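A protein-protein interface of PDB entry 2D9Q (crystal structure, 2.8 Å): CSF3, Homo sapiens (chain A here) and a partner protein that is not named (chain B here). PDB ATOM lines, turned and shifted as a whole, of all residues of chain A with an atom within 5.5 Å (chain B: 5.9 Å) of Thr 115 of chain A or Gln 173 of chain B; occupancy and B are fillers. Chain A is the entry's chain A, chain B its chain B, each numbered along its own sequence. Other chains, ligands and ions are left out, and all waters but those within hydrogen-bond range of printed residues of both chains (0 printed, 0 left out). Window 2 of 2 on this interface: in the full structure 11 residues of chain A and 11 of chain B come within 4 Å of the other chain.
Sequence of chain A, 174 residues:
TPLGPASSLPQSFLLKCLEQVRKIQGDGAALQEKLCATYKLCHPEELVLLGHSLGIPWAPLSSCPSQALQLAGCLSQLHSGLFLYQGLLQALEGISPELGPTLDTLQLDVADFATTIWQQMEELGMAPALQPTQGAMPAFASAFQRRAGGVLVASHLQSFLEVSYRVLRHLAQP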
ATOM      1  N   VAL A 110      -1.108  33.242  -8.117  1.00  0.00           N
ATOM      2  CA  VAL A 110      -2.077  32.222  -8.319  1.00  0.00           C
ATOM      3  C   VAL A 110      -1.873  31.631  -9.733  1.00  0.00           C
ATOM      4  O   VAL A 110      -1.868  30.440  -9.946  1.00  0.00           O
ATOM      5  CB  VAL A 110      -3.376  32.865  -8.238  1.00  0.00           C
ATOM      6  CG1 VAL A 110      -4.341  32.218  -9.250  1.00  0.00           C
ATOM      7  CG2 VAL A 110      -3.874  32.794  -6.775  1.00  0.00           C
ATOM      8  N   ALA A 111      -1.685  32.508 -10.692  1.00  0.00           N
ATOM      9  CA  ALA A 111      -1.429  32.080 -12.058  1.00  0.00           C
ATOM     10  C   ALA A 111      -0.356  31.064 -12.241  1.00  0.00           C
ATOM     11  O   ALA A 111      -0.406  30.213 -13.173  1.00  0.00           O
ATOM     12  CB  ALA A 111      -1.058  33.306 -12.898  1.00  0.00           C
ATOM     13  N   ASP A 112       0.633  31.218 -11.404  1.00  0.00           N
ATOM     14  CA  ASP A 112       1.826  30.476 -11.548  1.00  0.00           C
ATOM     15  C   ASP A 112       1.708  29.102 -10.873  1.00  0.00           C
ATOM     16  O   ASP A 112       2.350  28.155 -11.254  1.00  0.00           O
ATOM     17  CB  ASP A 112       2.926  31.275 -10.884  1.00  0.00           C
ATOM     18  CG  ASP A 112       3.618  32.241 -11.826  1.00  0.00           C
ATOM     19  OD1 ASP A 112       4.579  32.987 -11.456  1.00  0.00           O
ATOM     20  OD2 ASP A 112       3.255  32.284 -12.979  1.00  0.00           O
ATOM     21  N   PHE A 113       0.882  29.030  -9.843  1.00  0.00           N
ATOM     22  CA  PHE A 113       0.578  27.794  -9.135  1.00  0.00           C
ATOM     23  C   PHE A 113      -0.269  27.023 -10.024  1.00  0.00           C
ATOM     24  O   PHE A 113      -0.232  25.837 -10.076  1.00  0.00           O
ATOM     25  CB  PHE A 113      -0.313  28.091  -7.970  1.00  0.00           C
ATOM     26  CG  PHE A 113      -0.478  26.958  -7.003  1.00  0.00           C
ATOM     27  CD1 PHE A 113       0.474  25.997  -6.878  1.00  0.00           C
ATOM     28  CD2 PHE A 113      -1.570  26.916  -6.184  1.00  0.00           C
ATOM     29  CE1 PHE A 113       0.335  25.054  -6.007  1.00  0.00           C
ATOM     30  CE2 PHE A 113      -1.707  25.975  -5.350  1.00  0.00           C
ATOM     31  CZ  PHE A 113      -0.750  25.039  -5.243  1.00  0.00           C
ATOM     32  N   ALA A 114      -1.094  27.768 -10.704  1.00  0.00           N
ATOM     33  CA  ALA A 114      -1.970  27.249 -11.683  1.00  0.00           C
ATOM     34  C   ALA A 114      -1.171  26.575 -12.762  1.00  0.00           C
ATOM     35  O   ALA A 114      -1.482  25.419 -13.101  1.00  0.00           O
ATOM     36  CB  ALA A 114      -2.771  28.350 -12.246  1.00  0.00           C
ATOM     37  N   THR A 115      -0.158  27.215 -13.344  1.00  0.00           N
ATOM     38  CA  THR A 115       0.546  26.397 -14.318  1.00  0.00           C
ATOM     39  C   THR A 115       1.611  25.491 -13.680  1.00  0.00           C
ATOM     40  O   THR A 115       2.063  24.572 -14.278  1.00  0.00           O
ATOM     41  CB  THR A 115       1.038  27.182 -15.403  1.00  0.00           C
ATOM     42  OG1 THR A 115       1.934  28.124 -14.836  1.00  0.00           O
ATOM     43  CG2 THR A 115      -0.197  27.894 -16.052  1.00  0.00           C
ATOM     44  N   THR A 116       1.937  25.648 -12.429  1.00  0.00           N
ATOM     45  CA  THR A 116       2.900  24.701 -11.886  1.00  0.00           C
ATOM     46  C   THR A 116       2.348  23.321 -11.791  1.00  0.00           C
ATOM     47  O   THR A 116       3.077  22.356 -11.638  1.00  0.00           O
ATOM     48  CB  THR A 116       3.361  25.154 -10.555  1.00  0.00           C
ATOM     49  OG1 THR A 116       4.351  26.146 -10.819  1.00  0.00           O
ATOM     50  CG2 THR A 116       4.069  24.029  -9.766  1.00  0.00           C
ATOM     51  N   ILE A 117       1.040  23.261 -11.878  1.00  0.00           N
ATOM     52  CA  ILE A 117       0.315  22.045 -11.704  1.00  0.00           C
ATOM     53  C   ILE A 117       0.219  21.566 -13.107  1.00  0.00           C
ATOM     54  O   ILE A 117       0.749  20.564 -13.462  1.00  0.00           O
ATOM     55  CB  ILE A 117      -1.097  22.358 -11.095  1.00  0.00           C
ATOM     56  CG1 ILE A 117      -1.078  22.762  -9.583  1.00  0.00           C
ATOM     57  CG2 ILE A 117      -2.012  21.217 -11.206  1.00  0.00           C
ATOM     58  CD1 ILE A 117      -0.269  21.876  -8.582  1.00  0.00           C
ATOM     59  N   TRP A 118      -0.404  22.354 -13.942  1.00  0.00           N
ATOM     60  CA  TRP A 118      -0.667  21.955 -15.305  1.00  0.00           C
ATOM     61  C   TRP A 118       0.499  21.331 -15.929  1.00  0.00           C
ATOM     62  O   TRP A 118       0.348  20.406 -16.632  1.00  0.00           O
ATOM     63  CB  TRP A 118      -0.999  23.156 -16.135  1.00  0.00           C
ATOM     64  CG  TRP A 118      -1.405  22.870 -17.537  1.00  0.00           C
ATOM     65  CD1 TRP A 118      -0.649  23.103 -18.617  1.00  0.00           C
ATOM     66  CD2 TRP A 118      -2.707  22.375 -18.058  1.00  0.00           C
ATOM     67  NE1 TRP A 118      -1.351  22.803 -19.768  1.00  0.00           N
ATOM     68  CE2 TRP A 118      -2.616  22.364 -19.457  1.00  0.00           C
ATOM     69  CE3 TRP A 118      -3.929  21.950 -17.475  1.00  0.00           C
ATOM     70  CZ2 TRP A 118      -3.693  21.944 -20.306  1.00  0.00           C
ATOM     71  CZ3 TRP A 118      -5.010  21.528 -18.334  1.00  0.00           C
ATOM     72  CH2 TRP A 118      -4.867  21.539 -19.722  1.00  0.00           C
ATOM     73  N   GLN A 119       1.683  21.833 -15.711  1.00  0.00           N
ATOM     74  CA  GLN A 119       2.810  21.182 -16.341  1.00  0.00           C
ATOM     75  C   GLN A 119       3.013  19.830 -15.665  1.00  0.00           C
ATOM     76  O   GLN A 119       2.821  18.814 -16.316  1.00  0.00           O
ATOM     77  CB  GLN A 119       4.073  22.038 -16.345  1.00  0.00           C
ATOM     78  CG  GLN A 119       4.224  23.057 -17.530  1.00  0.00           C
ATOM     79  CD  GLN A 119       5.626  23.648 -17.447  1.00  0.00           C
ATOM     80  OE1 GLN A 119       6.363  23.222 -16.547  1.00  0.00           O
ATOM     81  NE2 GLN A 119       6.008  24.613 -18.334  1.00  0.00           N
ATOM     82  N   GLN A 120       3.332  19.761 -14.381  1.00  0.00           N
ATOM     83  CA  GLN A 120       3.348  18.437 -13.757  1.00  0.00           C
ATOM     84  C   GLN A 120       2.310  17.445 -14.340  1.00  0.00           C
ATOM     85  O   GLN A 120       2.569  16.242 -14.431  1.00  0.00           O
ATOM     86  CB  GLN A 120       3.068  18.537 -12.279  1.00  0.00           C
ATOM     87  CG  GLN A 120       3.313  17.255 -11.560  1.00  0.00           C
ATOM     88  CD  GLN A 120       4.689  16.807 -11.842  1.00  0.00           C
ATOM     89  OE1 GLN A 120       5.342  17.476 -12.618  1.00  0.00           O
ATOM     90  NE2 GLN A 120       5.159  15.703 -11.241  1.00  0.00           N
ATOM     91  N   GLN A 131      -5.520  23.133 -23.725  1.00  0.00           N
ATOM     92  CA  GLN A 131      -5.485  24.007 -22.523  1.00  0.00           C
ATOM     93  C   GLN A 131      -6.730  24.941 -22.381  1.00  0.00           C
ATOM     94  O   GLN A 131      -6.811  25.927 -23.103  1.00  0.00           O
ATOM     95  CB  GLN A 131      -4.171  24.846 -22.531  1.00  0.00           C
ATOM     96  CG  GLN A 131      -4.205  26.205 -21.733  1.00  0.00           C
ATOM     97  CD  GLN A 131      -4.163  26.071 -20.164  1.00  0.00           C
ATOM     98  OE1 GLN A 131      -3.195  25.540 -19.620  1.00  0.00           O
ATOM     99  NE2 GLN A 131      -5.196  26.593 -19.462  1.00  0.00           N
ATOM    100  N   SER B 139      11.051  29.370 -20.817  1.00  0.00           N
ATOM    101  CA  SER B 139      11.114  28.060 -21.406  1.00  0.00           C
ATOM    102  C   SER B 139      10.528  27.063 -20.493  1.00  0.00           C
ATOM    103  O   SER B 139       9.769  27.349 -19.551  1.00  0.00           O
ATOM    104  CB  SER B 139      12.559  27.685 -21.638  1.00  0.00           C
ATOM    105  OG  SER B 139      12.706  26.883 -22.809  1.00  0.00           O
ATOM    106  N   ARG B 140      10.893  25.842 -20.808  1.00  0.00           N
ATOM    107  CA  ARG B 140      10.883  24.757 -19.839  1.00  0.00           C
ATOM    108  C   ARG B 140      12.072  23.869 -20.121  1.00  0.00           C
ATOM    109  O   ARG B 140      12.711  23.933 -21.146  1.00  0.00           O
ATOM    110  CB  ARG B 140       9.561  23.972 -19.852  1.00  0.00           C
ATOM    111  CG  ARG B 140       9.236  23.485 -21.212  1.00  0.00           C
ATOM    112  CD  ARG B 140       7.857  22.803 -21.376  1.00  0.00           C
ATOM    113  NE  ARG B 140       8.001  21.634 -22.318  1.00  0.00           N
ATOM    114  CZ  ARG B 140       8.120  21.690 -23.690  1.00  0.00           C
ATOM    115  NH1 ARG B 140       8.056  22.847 -24.366  1.00  0.00           N
ATOM    116  NH2 ARG B 140       8.287  20.565 -24.388  1.00  0.00           N
ATOM    117  N   LEU B 170       8.112  34.173 -14.743  1.00  0.00           N
ATOM    118  CA  LEU B 170       7.189  33.087 -14.558  1.00  0.00           C
ATOM    119  C   LEU B 170       7.764  32.231 -13.431  1.00  0.00           C
ATOM    120  O   LEU B 170       8.425  31.212 -13.669  1.00  0.00           O
ATOM    121  CB  LEU B 170       7.214  32.340 -15.855  1.00  0.00           C
ATOM    122  CG  LEU B 170       6.087  31.477 -16.324  1.00  0.00           C
ATOM    123  CD1 LEU B 170       5.785  30.439 -15.211  1.00  0.00           C
ATOM    124  CD2 LEU B 170       4.916  32.517 -16.765  1.00  0.00           C
ATOM    125  N   LEU B 171       7.587  32.667 -12.204  1.00  0.00           N
ATOM    126  CA  LEU B 171       8.167  31.872 -11.145  1.00  0.00           C
ATOM    127  C   LEU B 171       7.953  30.357 -11.299  1.00  0.00           C
ATOM    128  O   LEU B 171       6.990  29.878 -11.986  1.00  0.00           O
ATOM    129  CB  LEU B 171       7.625  32.289  -9.815  1.00  0.00           C
ATOM    130  CG  LEU B 171       7.790  33.780  -9.564  1.00  0.00           C
ATOM    131  CD1 LEU B 171       6.582  34.195  -8.710  1.00  0.00           C
ATOM    132  CD2 LEU B 171       9.085  34.046  -8.850  1.00  0.00           C
ATOM    133  N   TYR B 172       8.859  29.614 -10.657  1.00  0.00           N
ATOM    134  CA  TYR B 172       8.791  28.128 -10.647  1.00  0.00           C
ATOM    135  C   TYR B 172       8.735  27.512 -12.025  1.00  0.00           C
ATOM    136  O   TYR B 172       7.832  26.786 -12.314  1.00  0.00           O
ATOM    137  CB  TYR B 172       7.554  27.636  -9.826  1.00  0.00           C
ATOM    138  CG  TYR B 172       7.646  28.023  -8.358  1.00  0.00           C
ATOM    139  CD1 TYR B 172       8.562  27.415  -7.472  1.00  0.00           C
ATOM    140  CD2 TYR B 172       6.910  29.105  -7.875  1.00  0.00           C
ATOM    141  CE1 TYR B 172       8.657  27.870  -6.143  1.00  0.00           C
ATOM    142  CE2 TYR B 172       7.007  29.530  -6.501  1.00  0.00           C
ATOM    143  CZ  TYR B 172       7.854  28.916  -5.672  1.00  0.00           C
ATOM    144  OH  TYR B 172       7.890  29.428  -4.401  1.00  0.00           O
ATOM    145  N   GLN B 173       9.681  27.858 -12.869  1.00  0.00           N
ATOM    146  CA  GLN B 173       9.756  27.447 -14.271  1.00  0.00           C
ATOM    147  C   GLN B 173      11.045  28.056 -14.765  1.00  0.00           C
ATOM    148  O   GLN B 173      11.622  28.931 -14.128  1.00  0.00           O
ATOM    149  CB  GLN B 173       8.646  28.019 -15.200  1.00  0.00           C
ATOM    150  CG  GLN B 173       7.524  27.022 -15.801  1.00  0.00           C
ATOM    151  CD  GLN B 173       6.532  26.544 -14.669  1.00  0.00           C
ATOM    152  OE1 GLN B 173       6.869  25.592 -13.955  1.00  0.00           O
ATOM    153  NE2 GLN B 173       5.379  27.259 -14.449  1.00  0.00           N
ATOM    154  N   ASN B 174      11.498  27.639 -15.938  1.00  0.00           N
ATOM    155  CA  ASN B 174      12.829  28.002 -16.331  1.00  0.00           C
ATOM    156  C   ASN B 174      12.789  28.847 -17.562  1.00  0.00           C
ATOM    157  O   ASN B 174      12.048  28.514 -18.575  1.00  0.00           O
ATOM    158  CB  ASN B 174      13.691  26.789 -16.658  1.00  0.00           C
ATOM    159  CG  ASN B 174      13.858  25.880 -15.544  1.00  0.00           C
ATOM    160  OD1 ASN B 174      14.288  26.230 -14.456  1.00  0.00           O
ATOM    161  ND2 ASN B 174      13.547  24.657 -15.813  1.00  0.00           N
ATOM    162  N   MET B 175      13.728  29.829 -17.462  1.00  0.00           N
ATOM    163  CA  MET B 175      13.948  30.806 -18.454  1.00  0.00           C
ATOM    164  C   MET B 175      15.380  30.878 -18.889  1.00  0.00           C
ATOM    165  O   MET B 175      16.282  30.522 -18.214  1.00  0.00           O
ATOM    166  CB  MET B 175      13.457  32.096 -17.894  1.00  0.00           C
ATOM    167  CG  MET B 175      14.085  32.560 -16.511  1.00  0.00           C
ATOM    168  SD  MET B 175      13.726  34.399 -16.346  1.00  0.00           S
ATOM    169  CE  MET B 175      11.953  34.196 -16.102  1.00  0.00           C
ATOM    170  N   LEU B 195      17.500  29.043 -15.700  1.00  0.00           N
ATOM    171  CA  LEU B 195      17.172  29.042 -14.282  1.00  0.00           C
ATOM    172  C   LEU B 195      15.671  29.319 -14.038  1.00  0.00           C
ATOM    173  O   LEU B 195      14.897  29.668 -14.986  1.00  0.00           O
ATOM    174  CB  LEU B 195      18.111  29.974 -13.484  1.00  0.00           C
ATOM    175  CG  LEU B 195      18.246  31.440 -13.960  1.00  0.00           C
ATOM    176  CD1 LEU B 195      16.879  31.958 -14.079  1.00  0.00           C
ATOM    177  CD2 LEU B 195      18.894  32.348 -13.054  1.00  0.00           C
ATOM    178  N   ASP B 196      15.322  29.052 -12.772  1.00  0.00           N
ATOM    179  CA  ASP B 196      14.050  29.307 -12.128  1.00  0.00           C
ATOM    180  C   ASP B 196      14.307  30.414 -11.102  1.00  0.00           C
ATOM    181  O   ASP B 196      15.017  30.224 -10.075  1.00  0.00           O
ATOM    182  CB  ASP B 196      13.660  28.056 -11.373  1.00  0.00           C
ATOM    183  CG  ASP B 196      12.364  28.195 -10.599  1.00  0.00           C
ATOM    184  OD1 ASP B 196      11.850  27.124 -10.131  1.00  0.00           O
ATOM    185  OD2 ASP B 196      11.766  29.305 -10.471  1.00  0.00           O
ATOM    186  N   PRO B 197      13.735  31.572 -11.355  1.00  0.00           N
ATOM    187  CA  PRO B 197      14.031  32.733 -10.558  1.00  0.00           C
ATOM    188  C   PRO B 197      13.989  32.342  -9.115  1.00  0.00           C
ATOM    189  O   PRO B 197      14.633  32.949  -8.265  1.00  0.00           O
ATOM    190  CB  PRO B 197      12.900  33.636 -10.920  1.00  0.00           C
ATOM    191  CG  PRO B 197      12.798  33.397 -12.322  1.00  0.00           C
ATOM    192  CD  PRO B 197      12.747  31.886 -12.378  1.00  0.00           C
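Of chain B, only Gln 173 comes within 4 Å of Thr 115 of chain A. Printed residues of chain A within 4 Å of Tyr 172 of chain B: Thr 116 (3.7 Å). Printed residues of chain A within 4 Å of Leu 171 of chain B: Asp 112 (3.1 Å). The nearest residue of chain A that does not touch Gln 173 of chain B is Asp 112 of chain A (4.5 Å).
The side-chain carboxylate of Asp 112 of chain A lies within hydrogen-bond range of the backbone NH of Leu 171 of chain B, 3.1 Å away.
Along chain A the printed residues that touch a printed residue of chain B span positions 112 to 119. Among the printed residues, no Asp or Glu carboxylate lies within 4 Å of a Lys or Arg side-chain nitrogen of the other chain.
OG1 of Thr 116 of chain A lies within hydrogen-bond range of O of Asp 112 of chain A (2.9 Å). OD2 of Asp 196 of chain B lies within hydrogen-bond range of N of Tyr 172 of chain B (2.9 Å). The backbone NH (N) of Gln 173 of chain B sits at hydrogen-bond distance from the side-chain carboxylate (OD2) of Asp 196 of chain B (3.5 Å).
Among the printed residues, merely in contact across the chains: Asp 112 of chain A with Leu 170 of chain B (3.8 Å), Thr 115 of chain A with Gln 173 of chain B (3.6 Å), Thr 116 of chain A with Tyr 172 of chain B (3.7 Å), Thr 116 of chain A with Gln 173 of chain B (3.9 Å), Gln 119 of chain A with Arg 140 of chain B (3.9 Å) and Gln 119 of chain A with Gln 173 of chain B (3.5 Å).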
